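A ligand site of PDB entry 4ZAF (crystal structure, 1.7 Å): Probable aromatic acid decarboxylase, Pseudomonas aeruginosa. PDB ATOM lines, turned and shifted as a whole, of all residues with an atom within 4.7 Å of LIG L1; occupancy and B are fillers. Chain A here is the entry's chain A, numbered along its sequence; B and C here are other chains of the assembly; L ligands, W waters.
The backbone carbonyl oxygen (O) of Cys 116 of chain B sits at hydrogen-bond distance from an oxygen (O5) of LIG L1. An oxygen (O9) of LIG L1 lies within hydrogen-bond range of the side-chain hydroxyl (OG1) of Thr 107 (2.6 Å). N of Gly 13 lies within hydrogen-bond range of O8 of LIG L1, at 2.7 Å. O of Arg 139 lies within hydrogen-bond range of N2 of LIG L1, at 3.0 Å. An oxygen (O1) of LIG L1 sits at hydrogen-bond distance from the backbone NH (N) of Thr 105, at 2.9 Å. NH2 of Arg 139 lies within salt-bridge range of O3 of LG2 L2 (3.1 Å). O3 of LIG L1 is in hydrogen-bond range of O of Gly 13, 2.6 Å away. An oxygen (O2) of LIG L1 sits at hydrogen-bond distance from the backbone NH of Ser 15, at 3.1 Å. The side-chain hydroxyl of Tyr 169 of chain C lies within hydrogen-bond range of an oxygen (O3) of LG2 L2 (2.8 Å). The guanidinium group of Arg 122 of chain B lies within hydrogen-bond range of an oxygen (O1) of LIG L1 (3.5 Å). OG of Ser 39 lies within hydrogen-bond range of O8 of LIG L1, 2.6 Å away. O9 of LIG L1 sits at hydrogen-bond distance from OG of Ser 104, at 2.5 Å. OG1 of Thr 105 sits at hydrogen-bond distance from O1 of LIG L1 (3.3 Å). O2 of LG2 L2 is in salt-bridge range of NH2 of Arg 122 of chain B, 3.0 Å away. NH2 of Arg 139 is in hydrogen-bond range of O2 of LIG L1, at 2.7 Å. An oxygen (O2) of LG2 L2 sits close to the side-chain carboxylate (OE1) of Glu 140.
The side-chain hydroxyl (OG) of Ser 104 lies close to the backbone NH (N) of Gly 106 (3.4 Å). OG of Ser 104 is in hydrogen-bond range of N of Thr 107 (2.9 Å). N of Ser 104 is in hydrogen-bond range of OG1 of Thr 12 (2.9 Å). OG of Ser 39 is in hydrogen-bond range of N of Ala 42, 3.0 Å away. The indole nitrogen (NE1) of Trp 200 of chain C is in hydrogen-bond range of the backbone carbonyl oxygen (O) of Trp 84 of chain B (3.0 Å). The backbone NH (N) of Tyr 169 of chain C is in hydrogen-bond range of the side-chain hydroxyl (OG) of Ser 15, at 3.4 Å. NH2 of Arg 139 lies within salt-bridge range of OE1 of Glu 140 (3.99 Å). The side-chain hydroxyl of Thr 105 sits at hydrogen-bond distance from the guanidinium group of Arg 122 of chain B (3.3 Å).
Thr 12 touches LIG L1 (CB to O8, 3.5 Å). Ala 14 touches LIG L1. Ala 41 touches LIG L1. CG2 of Val 45 touches C6 of LIG L1, 3.7 Å away. Glu 140 touches LIG L1 (OE2 to O1, 3.6 Å). Trp 84 of chain B touches LIG L1 (CB to C9, 3.3 Å). Met 85 of chain B touches LIG L1. Hydrophobic or aromatic side chains that line LIG L1: Ala 14, Ala 41, Val 45, Trp 84 of chain B and Met 85 of chain B. 16 residues have an atom within 4 Å of LIG L1: Thr 12, Gly 13, Ala 14, Ser 15, Ser 39, Ala 41, Val 45, Ser 104, Thr 105, Thr 107, Arg 139, Glu 140, Trp 84 of chain B, Met 85 of chain B, Cys 116 of chain B and Arg 122 of chain B. The nearest printed residue that does not touch LIG L1 is Thr 48 (4.1 Å).
Water W1 bridges an oxygen (O7) of LIG L1 (2.7 Å) and the side-chain amide oxygen of Asn 117 of chain B (3.3 Å). Water W6 lies within hydrogen-bond range of an oxygen (O4) of LIG L1 (2.8 Å), the side-chain hydroxyl of Thr 105 (2.9 Å), the backbone NH of Gly 106 (3.2 Å) and the side-chain sulfur of Cys 116 of chain B (3.8 Å). Water W4 lies within hydrogen-bond range of an oxygen (O7) of LIG L1 and the backbone NH (N) of Ala 41. Water W3 lies within hydrogen-bond range of OG1 of Thr 107, O9 of LIG L1 and O of Gly 106.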
ATOM      1  N   THR A  12       5.656   9.324  12.198  1.00  0.00           N
ATOM      2  CA  THR A  12       4.601   9.445  11.250  1.00  0.00           C
ATOM      3  C   THR A  12       3.649   8.230  11.324  1.00  0.00           C
ATOM      4  O   THR A  12       3.939   7.239  12.015  1.00  0.00           O
ATOM      5  CB  THR A  12       5.103   9.737   9.821  1.00  0.00           C
ATOM      6  OG1 THR A  12       5.808   8.593   9.309  1.00  0.00           O
ATOM      7  CG2 THR A  12       6.018  10.935   9.820  1.00  0.00           C
ATOM      8  N   GLY A  13       2.571   8.271  10.582  1.00  0.00           N
ATOM      9  CA  GLY A  13       1.447   7.386  10.815  1.00  0.00           C
ATOM     10  C   GLY A  13       1.513   5.973  10.220  1.00  0.00           C
ATOM     11  O   GLY A  13       0.497   5.490   9.756  1.00  0.00           O
ATOM     12  N   ALA A  14       2.665   5.328  10.293  1.00  0.00           N
ATOM     13  CA  ALA A  14       2.744   3.906  10.032  1.00  0.00           C
ATOM     14  C   ALA A  14       2.540   3.225  11.391  1.00  0.00           C
ATOM     15  O   ALA A  14       2.876   3.729  12.440  1.00  0.00           O
ATOM     16  CB  ALA A  14       4.103   3.514   9.486  1.00  0.00           C
ATOM     17  N   SER A  15       2.114   1.998  11.299  1.00  0.00           N
ATOM     18  CA  SER A  15       2.035   1.108  12.447  1.00  0.00           C
ATOM     19  C   SER A  15       3.437   0.939  12.954  1.00  0.00           C
ATOM     20  O   SER A  15       4.467   0.970  12.216  1.00  0.00           O
ATOM     21  CB  SER A  15       1.364  -0.197  12.045  1.00  0.00           C
ATOM     22  OG  SER A  15       1.142  -0.994  13.181  1.00  0.00           O
ATOM     23  N   SER A  39       3.178  13.537  13.427  1.00  0.00           N
ATOM     24  CA  SER A  39       2.123  13.894  12.545  1.00  0.00           C
ATOM     25  C   SER A  39       0.771  13.625  13.152  1.00  0.00           C
ATOM     26  O   SER A  39       0.673  12.856  14.089  1.00  0.00           O
ATOM     27  CB  SER A  39       2.220  13.081  11.237  1.00  0.00           C
ATOM     28  OG  SER A  39       1.869  11.736  11.452  1.00  0.00           O
ATOM     29  N   ALA A  41      -1.671  11.868  11.828  1.00  0.00           N
ATOM     30  CA  ALA A  41      -1.940  10.457  11.725  1.00  0.00           C
ATOM     31  C   ALA A  41      -1.168   9.600  12.747  1.00  0.00           C
ATOM     32  O   ALA A  41      -1.716   8.633  13.267  1.00  0.00           O
ATOM     33  CB  ALA A  41      -1.677   9.981  10.256  1.00  0.00           C
ATOM     34  N   ALA A  42       0.105   9.936  13.039  1.00  0.00           N
ATOM     35  CA  ALA A  42       0.877   9.239  14.027  1.00  0.00           C
ATOM     36  C   ALA A  42       0.201   9.358  15.436  1.00  0.00           C
ATOM     37  O   ALA A  42       0.250   8.376  16.211  1.00  0.00           O
ATOM     38  CB  ALA A  42       2.276   9.704  14.117  1.00  0.00           C
ATOM     39  N   VAL A  45      -2.360   6.677  15.325  1.00  0.00           N
ATOM     40  CA  VAL A  45      -1.719   5.400  15.488  1.00  0.00           C
ATOM     41  C   VAL A  45      -1.368   5.156  16.976  1.00  0.00           C
ATOM     42  O   VAL A  45      -1.594   4.059  17.507  1.00  0.00           O
ATOM     43  CB  VAL A  45      -0.475   5.234  14.580  1.00  0.00           C
ATOM     44  CG1 VAL A  45       0.190   3.904  14.828  1.00  0.00           C
ATOM     45  CG2 VAL A  45      -0.865   5.281  13.122  1.00  0.00           C
ATOM     46  N   THR A  48      -4.360   4.169  19.020  1.00  0.00           N
ATOM     47  CA  THR A  48      -4.827   2.808  18.628  1.00  0.00           C
ATOM     48  C   THR A  48      -3.948   1.684  19.109  1.00  0.00           C
ATOM     49  O   THR A  48      -4.416   0.640  19.551  1.00  0.00           O
ATOM     50  CB  THR A  48      -4.866   2.756  17.055  1.00  0.00           C
ATOM     51  OG1 THR A  48      -5.667   3.812  16.577  1.00  0.00           O
ATOM     52  CG2 THR A  48      -5.433   1.464  16.496  1.00  0.00           C
ATOM     53  N   SER A 104       5.656   6.427   7.447  1.00  0.00           N
ATOM     54  CA  SER A 104       4.556   6.042   6.577  1.00  0.00           C
ATOM     55  C   SER A 104       4.980   6.089   5.103  1.00  0.00           C
ATOM     56  O   SER A 104       5.937   6.774   4.731  1.00  0.00           O
ATOM     57  CB  SER A 104       3.385   6.970   6.740  1.00  0.00           C
ATOM     58  OG  SER A 104       3.672   8.241   6.198  1.00  0.00           O
ATOM     59  N   THR A 105       4.190   5.385   4.250  1.00  0.00           N
ATOM     60  CA  THR A 105       4.488   5.402   2.807  1.00  0.00           C
ATOM     61  C   THR A 105       4.276   6.840   2.302  1.00  0.00           C
ATOM     62  O   THR A 105       4.964   7.284   1.377  1.00  0.00           O
ATOM     63  CB  THR A 105       3.651   4.399   2.018  1.00  0.00           C
ATOM     64  OG1 THR A 105       2.273   4.627   2.223  1.00  0.00           O
ATOM     65  CG2 THR A 105       4.002   3.015   2.505  1.00  0.00           C
ATOM     66  N   GLY A 106       3.317   7.577   2.911  1.00  0.00           N
ATOM     67  CA  GLY A 106       3.090   8.961   2.479  1.00  0.00           C
ATOM     68  C   GLY A 106       4.194   9.884   2.826  1.00  0.00           C
ATOM     69  O   GLY A 106       4.534  10.761   2.012  1.00  0.00           O
ATOM     70  N   THR A 107       4.813   9.710   4.003  1.00  0.00           N
ATOM     71  CA  THR A 107       5.980  10.480   4.326  1.00  0.00           C
ATOM     72  C   THR A 107       7.194  10.118   3.518  1.00  0.00           C
ATOM     73  O   THR A 107       7.905  10.989   3.013  1.00  0.00           O
ATOM     74  CB  THR A 107       6.229  10.495   5.840  1.00  0.00           C
ATOM     75  OG1 THR A 107       5.161  11.303   6.449  1.00  0.00           O
ATOM     76  CG2 THR A 107       7.561  11.146   6.079  1.00  0.00           C
ATOM     77  N   ARG A 139       7.329   1.023   7.625  1.00  0.00           N
ATOM     78  CA  ARG A 139       6.575  -0.180   8.070  1.00  0.00           C
ATOM     79  C   ARG A 139       5.402  -0.390   7.131  1.00  0.00           C
ATOM     80  O   ARG A 139       4.455   0.381   7.176  1.00  0.00           O
ATOM     81  CB  ARG A 139       6.084  -0.023   9.533  1.00  0.00           C
ATOM     82  CG  ARG A 139       5.787  -1.330  10.325  1.00  0.00           C
ATOM     83  CD  ARG A 139       5.056  -2.456   9.602  1.00  0.00           C
ATOM     84  NE  ARG A 139       3.782  -2.075   9.173  1.00  0.00           N
ATOM     85  CZ  ARG A 139       2.926  -2.775   8.405  1.00  0.00           C
ATOM     86  NH1 ARG A 139       3.092  -4.026   7.983  1.00  0.00           N
ATOM     87  NH2 ARG A 139       1.857  -2.136   8.028  1.00  0.00           N
ATOM     88  N   GLU A 140       5.541  -1.342   6.234  1.00  0.00           N
ATOM     89  CA  GLU A 140       4.533  -1.574   5.218  1.00  0.00           C
ATOM     90  C   GLU A 140       4.794  -2.961   4.675  1.00  0.00           C
ATOM     91  O   GLU A 140       5.901  -3.437   4.685  1.00  0.00           O
ATOM     92  CB  GLU A 140       4.585  -0.483   4.125  1.00  0.00           C
ATOM     93  CG  GLU A 140       3.471  -0.628   3.050  1.00  0.00           C
ATOM     94  CD  GLU A 140       2.103  -0.587   3.615  1.00  0.00           C
ATOM     95  OE1 GLU A 140       1.622  -1.678   4.069  1.00  0.00           O
ATOM     96  OE2 GLU A 140       1.414   0.475   3.573  1.00  0.00           O
ATOM     97  N   TRP B  84      -9.145   6.702   8.598  1.00  0.00           N
ATOM     98  CA  TRP B  84      -8.235   5.578   8.485  1.00  0.00           C
ATOM     99  C   TRP B  84      -8.795   4.261   9.045  1.00  0.00           C
ATOM    100  O   TRP B  84      -8.270   3.213   8.793  1.00  0.00           O
ATOM    101  CB  TRP B  84      -6.868   5.908   9.124  1.00  0.00           C
ATOM    102  CG  TRP B  84      -6.330   7.259   8.739  1.00  0.00           C
ATOM    103  CD1 TRP B  84      -6.130   8.319   9.560  1.00  0.00           C
ATOM    104  CD2 TRP B  84      -5.990   7.708   7.432  1.00  0.00           C
ATOM    105  NE1 TRP B  84      -5.737   9.412   8.838  1.00  0.00           N
ATOM    106  CE2 TRP B  84      -5.620   9.053   7.525  1.00  0.00           C
ATOM    107  CE3 TRP B  84      -5.997   7.098   6.148  1.00  0.00           C
ATOM    108  CZ2 TRP B  84      -5.231   9.796   6.432  1.00  0.00           C
ATOM    109  CZ3 TRP B  84      -5.574   7.855   5.060  1.00  0.00           C
ATOM    110  CH2 TRP B  84      -5.290   9.181   5.199  1.00  0.00           C
ATOM    111  N   MET B  85      -9.907   4.317   9.764  1.00  0.00           N
ATOM    112  CA  MET B  85     -10.576   3.085  10.219  1.00  0.00           C
ATOM    113  C   MET B  85     -11.445   2.421   9.161  1.00  0.00           C
ATOM    114  O   MET B  85     -11.960   1.352   9.357  1.00  0.00           O
ATOM    115  CB  MET B  85     -11.443   3.451  11.490  1.00  0.00           C
ATOM    116  CG  MET B  85     -10.649   4.108  12.615  1.00  0.00           C
ATOM    117  SD  MET B  85      -8.913   3.549  12.970  1.00  0.00           S
ATOM    118  CE  MET B  85      -8.066   5.104  13.279  1.00  0.00           C
ATOM    119  N   CYS B 116       0.167  10.311   0.237  1.00  0.00           N
ATOM    120  CA  CYS B 116      -0.925   9.522   0.831  1.00  0.00           C
ATOM    121  C   CYS B 116      -1.789  10.346   1.658  1.00  0.00           C
ATOM    122  O   CYS B 116      -2.267   9.816   2.703  1.00  0.00           O
ATOM    123  CB  CYS B 116      -0.421   8.294   1.659  1.00  0.00           C
ATOM    124  SG  CYS B 116      -0.278   6.700   0.807  1.00  0.00           S
ATOM    125  N   ASN B 117      -2.090  11.565   1.148  1.00  0.00           N
ATOM    126  CA  ASN B 117      -2.584  12.638   1.967  1.00  0.00           C
ATOM    127  C   ASN B 117      -4.051  12.652   2.404  1.00  0.00           C
ATOM    128  O   ASN B 117      -4.478  13.573   3.121  1.00  0.00           O
ATOM    129  CB  ASN B 117      -2.262  14.033   1.385  1.00  0.00           C
ATOM    130  CG  ASN B 117      -0.724  14.336   1.423  1.00  0.00           C
ATOM    131  OD1 ASN B 117      -0.043  14.018   2.411  1.00  0.00           O
ATOM    132  ND2 ASN B 117      -0.192  14.908   0.365  1.00  0.00           N
ATOM    133  N   ARG B 122      -4.550   7.154  -0.162  1.00  0.00           N
ATOM    134  CA  ARG B 122      -4.119   5.971   0.542  1.00  0.00           C
ATOM    135  C   ARG B 122      -4.785   4.757  -0.010  1.00  0.00           C
ATOM    136  O   ARG B 122      -4.166   3.683  -0.114  1.00  0.00           O
ATOM    137  CB  ARG B 122      -4.395   6.098   2.051  1.00  0.00           C
ATOM    138  CG  ARG B 122      -4.093   4.852   2.884  1.00  0.00           C
ATOM    139  CD  ARG B 122      -2.669   4.361   2.850  1.00  0.00           C
ATOM    140  NE  ARG B 122      -2.559   3.168   3.654  1.00  0.00           N
ATOM    141  CZ  ARG B 122      -1.470   2.451   3.758  1.00  0.00           C
ATOM    142  NH1 ARG B 122      -0.340   2.793   3.088  1.00  0.00           N
ATOM    143  NH2 ARG B 122      -1.550   1.328   4.495  1.00  0.00           N
ATOM    144  N   TYR C 169      -1.193  -3.001  14.674  1.00  0.00           N
ATOM    145  CA  TYR C 169      -2.472  -2.391  14.865  1.00  0.00           C
ATOM    146  C   TYR C 169      -3.539  -3.387  15.345  1.00  0.00           C
ATOM    147  O   TYR C 169      -4.672  -2.995  15.551  1.00  0.00           O
ATOM    148  CB  TYR C 169      -2.911  -1.694  13.575  1.00  0.00           C
ATOM    149  CG  TYR C 169      -2.819  -2.484  12.265  1.00  0.00           C
ATOM    150  CD1 TYR C 169      -3.780  -3.394  11.894  1.00  0.00           C
ATOM    151  CD2 TYR C 169      -1.752  -2.304  11.387  1.00  0.00           C
ATOM    152  CE1 TYR C 169      -3.752  -4.028  10.676  1.00  0.00           C
ATOM    153  CE2 TYR C 169      -1.669  -3.001  10.192  1.00  0.00           C
ATOM    154  CZ  TYR C 169      -2.691  -3.819   9.809  1.00  0.00           C
ATOM    155  OH  TYR C 169      -2.599  -4.419   8.567  1.00  0.00           O
ATOM    156  N   TRP C 200      -9.687  -5.476   8.018  1.00  0.00           N
ATOM    157  CA  TRP C 200      -9.779  -4.153   8.524  1.00  0.00           C
ATOM    158  C   TRP C 200     -11.044  -3.387   8.125  1.00  0.00           C
ATOM    159  O   TRP C 200     -11.390  -3.326   6.963  1.00  0.00           O
ATOM    160  CB  TRP C 200      -8.551  -3.322   8.040  1.00  0.00           C
ATOM    161  CG  TRP C 200      -8.436  -1.972   8.591  1.00  0.00           C
ATOM    162  CD1 TRP C 200      -8.813  -0.788   7.990  1.00  0.00           C
ATOM    163  CD2 TRP C 200      -7.973  -1.596   9.878  1.00  0.00           C
ATOM    164  NE1 TRP C 200      -8.563   0.250   8.793  1.00  0.00           N
ATOM    165  CE2 TRP C 200      -8.077  -0.213   9.992  1.00  0.00           C
ATOM    166  CE3 TRP C 200      -7.464  -2.316  10.975  1.00  0.00           C
ATOM    167  CZ2 TRP C 200      -7.689   0.482  11.113  1.00  0.00           C
ATOM    168  CZ3 TRP C 200      -7.098  -1.620  12.102  1.00  0.00           C
ATOM    169  CH2 TRP C 200      -7.219  -0.243  12.187  1.00  0.00           C
HETATM  170  N1  LIG L   1       0.361   3.808   6.638  1.00  0.00           N
HETATM  171  C1  LIG L   1       1.534   3.117   6.295  1.00  0.00           C
HETATM  172  O1  LIG L   1       2.219   3.546   5.308  1.00  0.00           O
HETATM  173  N2  LIG L   1       1.941   2.016   6.949  1.00  0.00           N
HETATM  174  C2  LIG L   1       1.213   1.516   8.030  1.00  0.00           C
HETATM  175  O2  LIG L   1       1.628   0.523   8.664  1.00  0.00           O
HETATM  176  C3  LIG L   1       0.069   2.235   8.425  1.00  0.00           C
HETATM  177  N3  LIG L   1      -0.638   1.754   9.531  1.00  0.00           N
HETATM  178  C4  LIG L   1      -1.639   2.573   9.950  1.00  0.00           C
HETATM  179  C5  LIG L   1      -2.306   2.187  11.128  1.00  0.00           C
HETATM  180  C6  LIG L   1      -3.360   2.961  11.615  1.00  0.00           C
HETATM  181  C7  LIG L   1      -4.057   2.519  12.829  1.00  0.00           C
HETATM  182  C8  LIG L   1      -3.730   4.105  10.978  1.00  0.00           C
HETATM  183  C9  LIG L   1      -4.831   4.899  11.460  1.00  0.00           C
HETATM  184  C10 LIG L   1      -3.114   4.501   9.746  1.00  0.00           C
HETATM  185  C11 LIG L   1      -2.056   3.726   9.237  1.00  0.00           C
HETATM  186  N4  LIG L   1      -1.420   4.032   8.073  1.00  0.00           N
HETATM  187  C12 LIG L   1      -0.366   3.369   7.733  1.00  0.00           C
HETATM  188  C13 LIG L   1      -1.911   5.179   7.248  1.00  0.00           C
HETATM  189  C14 LIG L   1      -1.451   6.569   7.361  1.00  0.00           C
HETATM  190  O3  LIG L   1      -1.455   6.899   8.703  1.00  0.00           O
HETATM  191  C15 LIG L   1      -1.916   7.454   6.277  1.00  0.00           C
HETATM  192  O4  LIG L   1      -1.576   7.074   4.914  1.00  0.00           O
HETATM  193  C16 LIG L   1      -1.438   8.842   6.583  1.00  0.00           C
HETATM  194  O5  LIG L   1      -1.891   9.719   5.488  1.00  0.00           O
HETATM  195  C17 LIG L   1       0.025   8.999   6.864  1.00  0.00           C
HETATM  196  O6  LIG L   1       0.204  10.408   7.121  1.00  0.00           O
HETATM  197  P1  LIG L   1       1.572  10.941   7.778  1.00  0.00           P
HETATM  198  O7  LIG L   1       1.428  12.488   7.739  1.00  0.00           O
HETATM  199  O8  LIG L   1       1.773  10.389   9.188  1.00  0.00           O
HETATM  200  O9  LIG L   1       2.724  10.468   6.819  1.00  0.00           O
HETATM  201  O1  LG2 L   2      -1.916  -2.824   4.571  1.00  0.00           O
HETATM  202  P1  LG2 L   2      -1.385  -2.244   5.850  1.00  0.00           P
HETATM  203  O2  LG2 L   2      -0.293  -1.171   5.508  1.00  0.00           O
HETATM  204  O3  LG2 L   2      -0.757  -3.165   6.839  1.00  0.00           O
HETATM  205  O4  LG2 L   2      -2.543  -1.366   6.530  1.00  0.00           O
HETATM  206  C1  LG2 L   2      -2.086  -0.536   7.603  1.00  0.00           C
HETATM  207  C2  LG2 L   2      -3.066   0.650   7.601  1.00  0.00           C
HETATM  208  C3  LG2 L   2      -4.246   0.654   8.525  1.00  0.00           C
HETATM  209  C4  LG2 L   2      -4.455  -0.449   9.549  1.00  0.00           C
HETATM  210  C5  LG2 L   2      -5.207   1.827   8.400  1.00  0.00           C
HETATM  211  O   HOH W   1       0.088  13.551   5.646  1.00  0.00           O
HETATM  212  O   HOH W   2       0.871  10.854   4.115  1.00  0.00           O
HETATM  213  O   HOH W   3       3.153  12.787   4.497  1.00  0.00           O
HETATM  214  O   HOH W   4      -0.760  13.229   9.314  1.00  0.00           O
HETATM  215  O   HOH W   5      -2.541  12.276   5.780  1.00  0.00           O
HETATM  216  O   HOH W   6       0.900   5.996   4.347  1.00  0.00           O
